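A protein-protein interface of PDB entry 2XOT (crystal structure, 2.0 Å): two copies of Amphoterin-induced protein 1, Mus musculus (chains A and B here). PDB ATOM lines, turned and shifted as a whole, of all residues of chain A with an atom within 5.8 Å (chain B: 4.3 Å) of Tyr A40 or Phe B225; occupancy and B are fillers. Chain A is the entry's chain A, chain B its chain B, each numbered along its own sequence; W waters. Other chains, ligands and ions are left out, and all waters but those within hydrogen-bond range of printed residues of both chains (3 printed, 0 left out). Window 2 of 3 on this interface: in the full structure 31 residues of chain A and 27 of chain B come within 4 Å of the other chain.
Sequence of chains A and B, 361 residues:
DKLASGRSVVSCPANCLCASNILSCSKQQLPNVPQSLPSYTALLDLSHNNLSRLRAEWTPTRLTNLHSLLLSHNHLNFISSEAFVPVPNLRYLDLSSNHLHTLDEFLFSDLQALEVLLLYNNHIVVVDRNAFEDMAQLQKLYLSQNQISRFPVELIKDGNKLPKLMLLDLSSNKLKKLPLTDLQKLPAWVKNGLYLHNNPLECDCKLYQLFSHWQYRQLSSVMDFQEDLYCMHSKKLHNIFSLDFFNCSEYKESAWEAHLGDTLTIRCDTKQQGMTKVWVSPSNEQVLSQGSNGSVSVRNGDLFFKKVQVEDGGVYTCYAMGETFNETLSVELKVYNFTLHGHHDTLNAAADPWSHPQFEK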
ATOM      1  N   VAL A   9     -18.954   3.826 -18.342  1.00  0.00           N
ATOM      2  CA  VAL A   9     -20.138   3.004 -18.074  1.00  0.00           C
ATOM      3  C   VAL A   9     -20.284   1.971 -19.201  1.00  0.00           C
ATOM      4  O   VAL A   9     -20.322   2.321 -20.371  1.00  0.00           O
ATOM      5  CB  VAL A   9     -21.403   3.889 -17.961  1.00  0.00           C
ATOM      6  CG1 VAL A   9     -22.694   3.059 -17.794  1.00  0.00           C
ATOM      7  CG2 VAL A   9     -21.229   4.891 -16.833  1.00  0.00           C
ATOM      8  N   SER A  11     -22.647  -0.058 -20.257  1.00  0.00           N
ATOM      9  CA  SER A  11     -23.851   0.024 -21.078  1.00  0.00           C
ATOM     10  C   SER A  11     -23.939   1.290 -21.942  1.00  0.00           C
ATOM     11  O   SER A  11     -24.839   1.392 -22.781  1.00  0.00           O
ATOM     12  CB  SER A  11     -25.116  -0.052 -20.206  1.00  0.00           C
ATOM     13  OG  SER A  11     -25.139   0.947 -19.202  1.00  0.00           O
ATOM     14  N   CYS A  12     -23.025   2.244 -21.760  1.00  0.00           N
ATOM     15  CA  CYS A  12     -23.137   3.520 -22.468  1.00  0.00           C
ATOM     16  C   CYS A  12     -22.792   3.357 -23.952  1.00  0.00           C
ATOM     17  O   CYS A  12     -21.673   2.969 -24.274  1.00  0.00           O
ATOM     18  CB  CYS A  12     -22.223   4.565 -21.838  1.00  0.00           C
ATOM     19  SG  CYS A  12     -22.576   6.250 -22.355  1.00  0.00           S
ATOM     20  N   CYS A  18     -23.498   9.294 -20.645  1.00  0.00           N
ATOM     21  CA  CYS A  18     -24.561   8.605 -19.920  1.00  0.00           C
ATOM     22  C   CYS A  18     -24.654   9.082 -18.481  1.00  0.00           C
ATOM     23  O   CYS A  18     -23.720   8.894 -17.697  1.00  0.00           O
ATOM     24  CB  CYS A  18     -24.334   7.086 -20.003  1.00  0.00           C
ATOM     25  SG  CYS A  18     -24.510   6.469 -21.695  1.00  0.00           S
ATOM     26  N   SER A  20     -26.964   8.177 -15.686  1.00  0.00           N
ATOM     27  CA  SER A  20     -27.944   7.161 -15.316  1.00  0.00           C
ATOM     28  C   SER A  20     -28.987   6.973 -16.420  1.00  0.00           C
ATOM     29  O   SER A  20     -28.659   6.478 -17.498  1.00  0.00           O
ATOM     30  CB  SER A  20     -28.553   7.429 -13.928  1.00  0.00           C
ATOM     31  OG  SER A  20     -29.303   8.618 -13.891  1.00  0.00           O
ATOM     32  N   ASN A  21     -30.232   7.375 -16.194  1.00  0.00           N
ATOM     33  CA  ASN A  21     -31.255   7.196 -17.238  1.00  0.00           C
ATOM     34  C   ASN A  21     -31.331   8.328 -18.309  1.00  0.00           C
ATOM     35  O   ASN A  21     -32.233   8.320 -19.150  1.00  0.00           O
ATOM     36  CB  ASN A  21     -32.616   6.894 -16.608  1.00  0.00           C
ATOM     37  CG  ASN A  21     -33.177   8.037 -15.810  1.00  0.00           C
ATOM     38  OD1 ASN A  21     -32.559   9.097 -15.675  1.00  0.00           O
ATOM     39  ND2 ASN A  21     -34.367   7.830 -15.267  1.00  0.00           N
ATOM     40  N   LEU A  23     -29.279   9.923 -21.602  1.00  0.00           N
ATOM     41  CA  LEU A  23     -28.209   9.738 -22.600  1.00  0.00           C
ATOM     42  C   LEU A  23     -28.120  10.998 -23.438  1.00  0.00           C
ATOM     43  O   LEU A  23     -29.064  11.349 -24.168  1.00  0.00           O
ATOM     44  CB  LEU A  23     -28.466   8.553 -23.522  1.00  0.00           C
ATOM     45  CG  LEU A  23     -27.907   7.185 -23.139  1.00  0.00           C
ATOM     46  CD1 LEU A  23     -28.315   6.770 -21.710  1.00  0.00           C
ATOM     47  CD2 LEU A  23     -28.383   6.157 -24.213  1.00  0.00           C
ATOM     48  N   PRO A  38     -29.440   1.207 -24.141  1.00  0.00           N
ATOM     49  CA  PRO A  38     -29.964   0.472 -22.987  1.00  0.00           C
ATOM     50  C   PRO A  38     -31.451   0.668 -22.698  1.00  0.00           C
ATOM     51  O   PRO A  38     -32.026   1.767 -22.878  1.00  0.00           O
ATOM     52  CB  PRO A  38     -29.130   0.993 -21.816  1.00  0.00           C
ATOM     53  CG  PRO A  38     -28.627   2.325 -22.251  1.00  0.00           C
ATOM     54  CD  PRO A  38     -28.493   2.264 -23.744  1.00  0.00           C
ATOM     55  N   SER A  39     -32.037  -0.399 -22.163  1.00  0.00           N
ATOM     56  CA  SER A  39     -33.462  -0.466 -21.931  1.00  0.00           C
ATOM     57  C   SER A  39     -33.915   0.453 -20.799  1.00  0.00           C
ATOM     58  O   SER A  39     -35.102   0.783 -20.725  1.00  0.00           O
ATOM     59  CB  SER A  39     -33.852  -1.925 -21.642  1.00  0.00           C
ATOM     60  OG  SER A  39     -33.175  -2.388 -20.487  1.00  0.00           O
ATOM     61  N   TYR A  40     -32.986   0.861 -19.929  1.00  0.00           N
ATOM     62  CA  TYR A  40     -33.278   1.813 -18.831  1.00  0.00           C
ATOM     63  C   TYR A  40     -33.386   3.289 -19.269  1.00  0.00           C
ATOM     64  O   TYR A  40     -33.757   4.151 -18.467  1.00  0.00           O
ATOM     65  CB  TYR A  40     -32.245   1.705 -17.687  1.00  0.00           C
ATOM     66  CG  TYR A  40     -30.811   2.010 -18.086  1.00  0.00           C
ATOM     67  CD1 TYR A  40     -30.429   3.298 -18.474  1.00  0.00           C
ATOM     68  CD2 TYR A  40     -29.830   1.011 -18.068  1.00  0.00           C
ATOM     69  CE1 TYR A  40     -29.136   3.575 -18.884  1.00  0.00           C
ATOM     70  CE2 TYR A  40     -28.514   1.290 -18.451  1.00  0.00           C
ATOM     71  CZ  TYR A  40     -28.175   2.578 -18.856  1.00  0.00           C
ATOM     72  OH  TYR A  40     -26.873   2.891 -19.232  1.00  0.00           O
ATOM     73  N   THR A  41     -33.071   3.576 -20.523  1.00  0.00           N
ATOM     74  CA  THR A  41     -33.056   4.954 -21.034  1.00  0.00           C
ATOM     75  C   THR A  41     -34.433   5.636 -20.882  1.00  0.00           C
ATOM     76  O   THR A  41     -35.472   5.106 -21.308  1.00  0.00           O
ATOM     77  CB  THR A  41     -32.563   4.980 -22.494  1.00  0.00           C
ATOM     78  OG1 THR A  41     -31.358   4.225 -22.594  1.00  0.00           O
ATOM     79  CG2 THR A  41     -32.320   6.393 -22.997  1.00  0.00           C
ATOM     80  N   ALA A  42     -34.426   6.801 -20.225  1.00  0.00           N
ATOM     81  CA  ALA A  42     -35.618   7.612 -19.989  1.00  0.00           C
ATOM     82  C   ALA A  42     -35.688   8.833 -20.899  1.00  0.00           C
ATOM     83  O   ALA A  42     -36.776   9.255 -21.317  1.00  0.00           O
ATOM     84  CB  ALA A  42     -35.657   8.060 -18.514  1.00  0.00           C
ATOM     85  N   ASN A  65     -39.056   2.347 -21.111  1.00  0.00           N
ATOM     86  CA  ASN A  65     -38.836   3.399 -20.144  1.00  0.00           C
ATOM     87  C   ASN A  65     -38.622   4.802 -20.738  1.00  0.00           C
ATOM     88  O   ASN A  65     -38.571   5.794 -20.001  1.00  0.00           O
ATOM     89  CB  ASN A  65     -37.636   3.032 -19.274  1.00  0.00           C
ATOM     90  CG  ASN A  65     -37.872   1.783 -18.457  1.00  0.00           C
ATOM     91  OD1 ASN A  65     -37.158   0.786 -18.599  1.00  0.00           O
ATOM     92  ND2 ASN A  65     -38.903   1.816 -17.626  1.00  0.00           N
ATOM     93  N   TYR B 195     -28.091   6.522  -7.367  1.00  0.00           N
ATOM     94  CA  TYR B 195     -27.159   5.908  -8.308  1.00  0.00           C
ATOM     95  C   TYR B 195     -25.710   6.169  -7.866  1.00  0.00           C
ATOM     96  O   TYR B 195     -25.269   7.313  -7.752  1.00  0.00           O
ATOM     97  CB  TYR B 195     -27.409   6.372  -9.762  1.00  0.00           C
ATOM     98  CG  TYR B 195     -28.786   6.049 -10.348  1.00  0.00           C
ATOM     99  CD1 TYR B 195     -29.045   4.816 -10.950  1.00  0.00           C
ATOM    100  CD2 TYR B 195     -29.809   6.971 -10.334  1.00  0.00           C
ATOM    101  CE1 TYR B 195     -30.286   4.518 -11.495  1.00  0.00           C
ATOM    102  CE2 TYR B 195     -31.065   6.666 -10.861  1.00  0.00           C
ATOM    103  CZ  TYR B 195     -31.298   5.443 -11.433  1.00  0.00           C
ATOM    104  OH  TYR B 195     -32.527   5.149 -11.971  1.00  0.00           O
ATOM    105  N   HIS B 197     -23.000   3.985  -9.091  1.00  0.00           N
ATOM    106  CA  HIS B 197     -22.157   3.123  -9.924  1.00  0.00           C
ATOM    107  C   HIS B 197     -21.025   3.948 -10.544  1.00  0.00           C
ATOM    108  O   HIS B 197     -21.098   5.175 -10.630  1.00  0.00           O
ATOM    109  CB  HIS B 197     -22.965   2.399 -11.029  1.00  0.00           C
ATOM    110  CG  HIS B 197     -23.745   3.319 -11.906  1.00  0.00           C
ATOM    111  ND1 HIS B 197     -23.268   3.780 -13.121  1.00  0.00           N
ATOM    112  CD2 HIS B 197     -24.940   3.920 -11.718  1.00  0.00           C
ATOM    113  CE1 HIS B 197     -24.150   4.609 -13.644  1.00  0.00           C
ATOM    114  NE2 HIS B 197     -25.170   4.715 -12.813  1.00  0.00           N
ATOM    115  N   SER B 221     -31.729   1.226  -9.303  1.00  0.00           N
ATOM    116  CA  SER B 221     -30.372   1.750  -9.107  1.00  0.00           C
ATOM    117  C   SER B 221     -29.319   0.623  -9.162  1.00  0.00           C
ATOM    118  O   SER B 221     -28.178   0.849  -9.566  1.00  0.00           O
ATOM    119  CB  SER B 221     -30.291   2.528  -7.779  1.00  0.00           C
ATOM    120  OG  SER B 221     -30.647   1.728  -6.655  1.00  0.00           O
ATOM    121  N   VAL B 222     -29.711  -0.586  -8.758  1.00  0.00           N
ATOM    122  CA  VAL B 222     -28.853  -1.767  -8.876  1.00  0.00           C
ATOM    123  C   VAL B 222     -29.127  -2.573 -10.154  1.00  0.00           C
ATOM    124  O   VAL B 222     -28.207  -2.856 -10.923  1.00  0.00           O
ATOM    125  CB  VAL B 222     -29.011  -2.681  -7.638  1.00  0.00           C
ATOM    126  CG1 VAL B 222     -28.410  -4.059  -7.897  1.00  0.00           C
ATOM    127  CG2 VAL B 222     -28.354  -2.039  -6.423  1.00  0.00           C
ATOM    128  N   MET B 223     -30.382  -2.932 -10.397  1.00  0.00           N
ATOM    129  CA  MET B 223     -30.722  -3.752 -11.572  1.00  0.00           C
ATOM    130  C   MET B 223     -30.257  -3.126 -12.908  1.00  0.00           C
ATOM    131  O   MET B 223     -29.750  -3.830 -13.781  1.00  0.00           O
ATOM    132  CB  MET B 223     -32.220  -4.048 -11.621  1.00  0.00           C
ATOM    133  CG  MET B 223     -32.758  -4.785 -10.412  1.00  0.00           C
ATOM    134  SD  MET B 223     -31.853  -6.271  -9.938  1.00  0.00           S
ATOM    135  CE  MET B 223     -30.768  -5.568  -8.746  1.00  0.00           C
ATOM    136  N   ASP B 224     -30.381  -1.814 -13.065  1.00  0.00           N
ATOM    137  CA  ASP B 224     -29.996  -1.189 -14.336  1.00  0.00           C
ATOM    138  C   ASP B 224     -28.464  -1.102 -14.554  1.00  0.00           C
ATOM    139  O   ASP B 224     -28.020  -0.936 -15.678  1.00  0.00           O
ATOM    140  CB  ASP B 224     -30.614   0.207 -14.450  1.00  0.00           C
ATOM    141  CG  ASP B 224     -32.113   0.188 -14.484  1.00  0.00           C
ATOM    142  OD1 ASP B 224     -32.694  -0.851 -14.778  1.00  0.00           O
ATOM    143  OD2 ASP B 224     -32.729   1.229 -14.235  1.00  0.00           O
ATOM    144  N   PHE B 225     -27.679  -1.249 -13.495  1.00  0.00           N
ATOM    145  CA  PHE B 225     -26.249  -0.919 -13.501  1.00  0.00           C
ATOM    146  C   PHE B 225     -25.359  -1.887 -12.751  1.00  0.00           C
ATOM    147  O   PHE B 225     -24.253  -1.519 -12.329  1.00  0.00           O
ATOM    148  CB  PHE B 225     -26.064   0.484 -12.917  1.00  0.00           C
ATOM    149  CG  PHE B 225     -26.719   1.541 -13.739  1.00  0.00           C
ATOM    150  CD1 PHE B 225     -26.154   1.940 -14.937  1.00  0.00           C
ATOM    151  CD2 PHE B 225     -27.907   2.128 -13.338  1.00  0.00           C
ATOM    152  CE1 PHE B 225     -26.764   2.903 -15.726  1.00  0.00           C
ATOM    153  CE2 PHE B 225     -28.512   3.080 -14.135  1.00  0.00           C
ATOM    154  CZ  PHE B 225     -27.931   3.470 -15.315  1.00  0.00           C
ATOM    155  N   GLN B 226     -25.806  -3.135 -12.611  1.00  0.00           N
ATOM    156  CA  GLN B 226     -25.054  -4.131 -11.841  1.00  0.00           C
ATOM    157  C   GLN B 226     -23.573  -4.235 -12.273  1.00  0.00           C
ATOM    158  O   GLN B 226     -22.683  -4.352 -11.434  1.00  0.00           O
ATOM    159  CB  GLN B 226     -25.716  -5.502 -11.968  1.00  0.00           C
ATOM    160  CG  GLN B 226     -27.004  -5.615 -11.232  1.00  0.00           C
ATOM    161  CD  GLN B 226     -27.620  -6.999 -11.375  1.00  0.00           C
ATOM    162  OE1 GLN B 226     -28.218  -7.317 -12.411  1.00  0.00           O
ATOM    163  NE2 GLN B 226     -27.467  -7.825 -10.347  1.00  0.00           N
ATOM    164  N   GLU B 227     -23.343  -4.182 -13.577  1.00  0.00           N
ATOM    165  CA  GLU B 227     -22.014  -4.309 -14.160  1.00  0.00           C
ATOM    166  C   GLU B 227     -21.123  -3.075 -13.888  1.00  0.00           C
ATOM    167  O   GLU B 227     -19.911  -3.143 -14.073  1.00  0.00           O
ATOM    168  CB  GLU B 227     -22.127  -4.539 -15.684  1.00  0.00           C
ATOM    169  N   ASP B 228     -21.700  -1.949 -13.471  1.00  0.00           N
ATOM    170  CA  ASP B 228     -20.878  -0.747 -13.172  1.00  0.00           C
ATOM    171  C   ASP B 228     -20.724  -0.434 -11.676  1.00  0.00           C
ATOM    172  O   ASP B 228     -20.098   0.580 -11.294  1.00  0.00           O
ATOM    173  CB  ASP B 228     -21.417   0.468 -13.927  1.00  0.00           C
ATOM    174  CG  ASP B 228     -21.311   0.306 -15.423  1.00  0.00           C
ATOM    175  OD1 ASP B 228     -20.178   0.116 -15.931  1.00  0.00           O
ATOM    176  OD2 ASP B 228     -22.368   0.361 -16.089  1.00  0.00           O
ATOM    177  N   LEU B 229     -21.291  -1.302 -10.838  1.00  0.00           N
ATOM    178  CA  LEU B 229     -21.184  -1.189  -9.392  1.00  0.00           C
ATOM    179  C   LEU B 229     -19.936  -1.894  -8.940  1.00  0.00           C
ATOM    180  O   LEU B 229     -19.933  -3.088  -8.699  1.00  0.00           O
ATOM    181  CB  LEU B 229     -22.416  -1.742  -8.673  1.00  0.00           C
ATOM    182  CG  LEU B 229     -23.598  -0.780  -8.722  1.00  0.00           C
ATOM    183  CD1 LEU B 229     -24.912  -1.451  -8.352  1.00  0.00           C
ATOM    184  CD2 LEU B 229     -23.347   0.399  -7.840  1.00  0.00           C
HETATM  185  O   HOH W   1     -24.745   6.091 -15.966  1.00  0.00           O
HETATM  186  O   HOH W   2     -34.666  -1.343 -17.512  1.00  0.00           O
HETATM  187  O   HOH W   3     -24.445  -0.869 -17.084  1.00  0.00           O
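OG of Ser A11 sits at hydrogen-bond distance from OH of Tyr A40 (2.6 Å).
The side-chain sulfur (SG) of Cys A12 forms a disulfide with the side-chain sulfur (SG) of Cys A18 (2.1 Å).
CG1 of Val A9 touches OD2 of Asp B228 (3.2 Å).
CB of Ser A20 touches CD2 of Tyr B195, at 3.8 Å.
Phe B225 touches Ser A20.
OD2 of Asp B224 touches CB of Tyr A40, 3.5 Å away.
CZ of Tyr A40 touches CE1 of Phe B225, 3.4 Å away.
Printed residues of chain B within 4 Å of Val A9: Asp B228.
Of the printed residues of chain B, Ser A20 touches Tyr B195 and Phe B225.
Tyr A40 touches just these residues of chain B: Asp B224 and Phe B225.
Of the printed residues of chain A, Tyr B195 touches Ser A20 (3.8 Å).
Of the printed residues of chain A, Asp B224 touches Tyr A40.
Of chain A, only Ser A20 and Tyr A40 come within 4 Å of Phe B225.
The nearest printed residue of chain B that does not touch Tyr A40 is Asp B228 (6.0 Å).
Of the 13 printed residues of chain A, 3 touch a printed residue of chain B.
Hydrophobic or aromatic side chains of chain A within 4 Å of the printed part of chain B: Val A9 and Tyr A40.
Of the 11 printed residues of chain B, 4 touch a printed residue of chain A.
No position is printed for both chains.
Water W3 bridges the side-chain carboxylate of Asp B228 and the side-chain hydroxyl of Ser A11.
Water W1 lies within hydrogen-bond range of the backbone NH (N) of Ser A20 (3.1 Å), the backbone carbonyl oxygen (O) of Cys A18 (3.5 Å) and a ring nitrogen (NE2) of His B197 (3.5 Å).
Water W2 lies within hydrogen-bond range of the side-chain carboxylate of Asp B224 (3.4 Å), the side-chain amide oxygen of Asn A65 (3.5 Å) and the side-chain hydroxyl of Ser A39 (3.5 Å).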
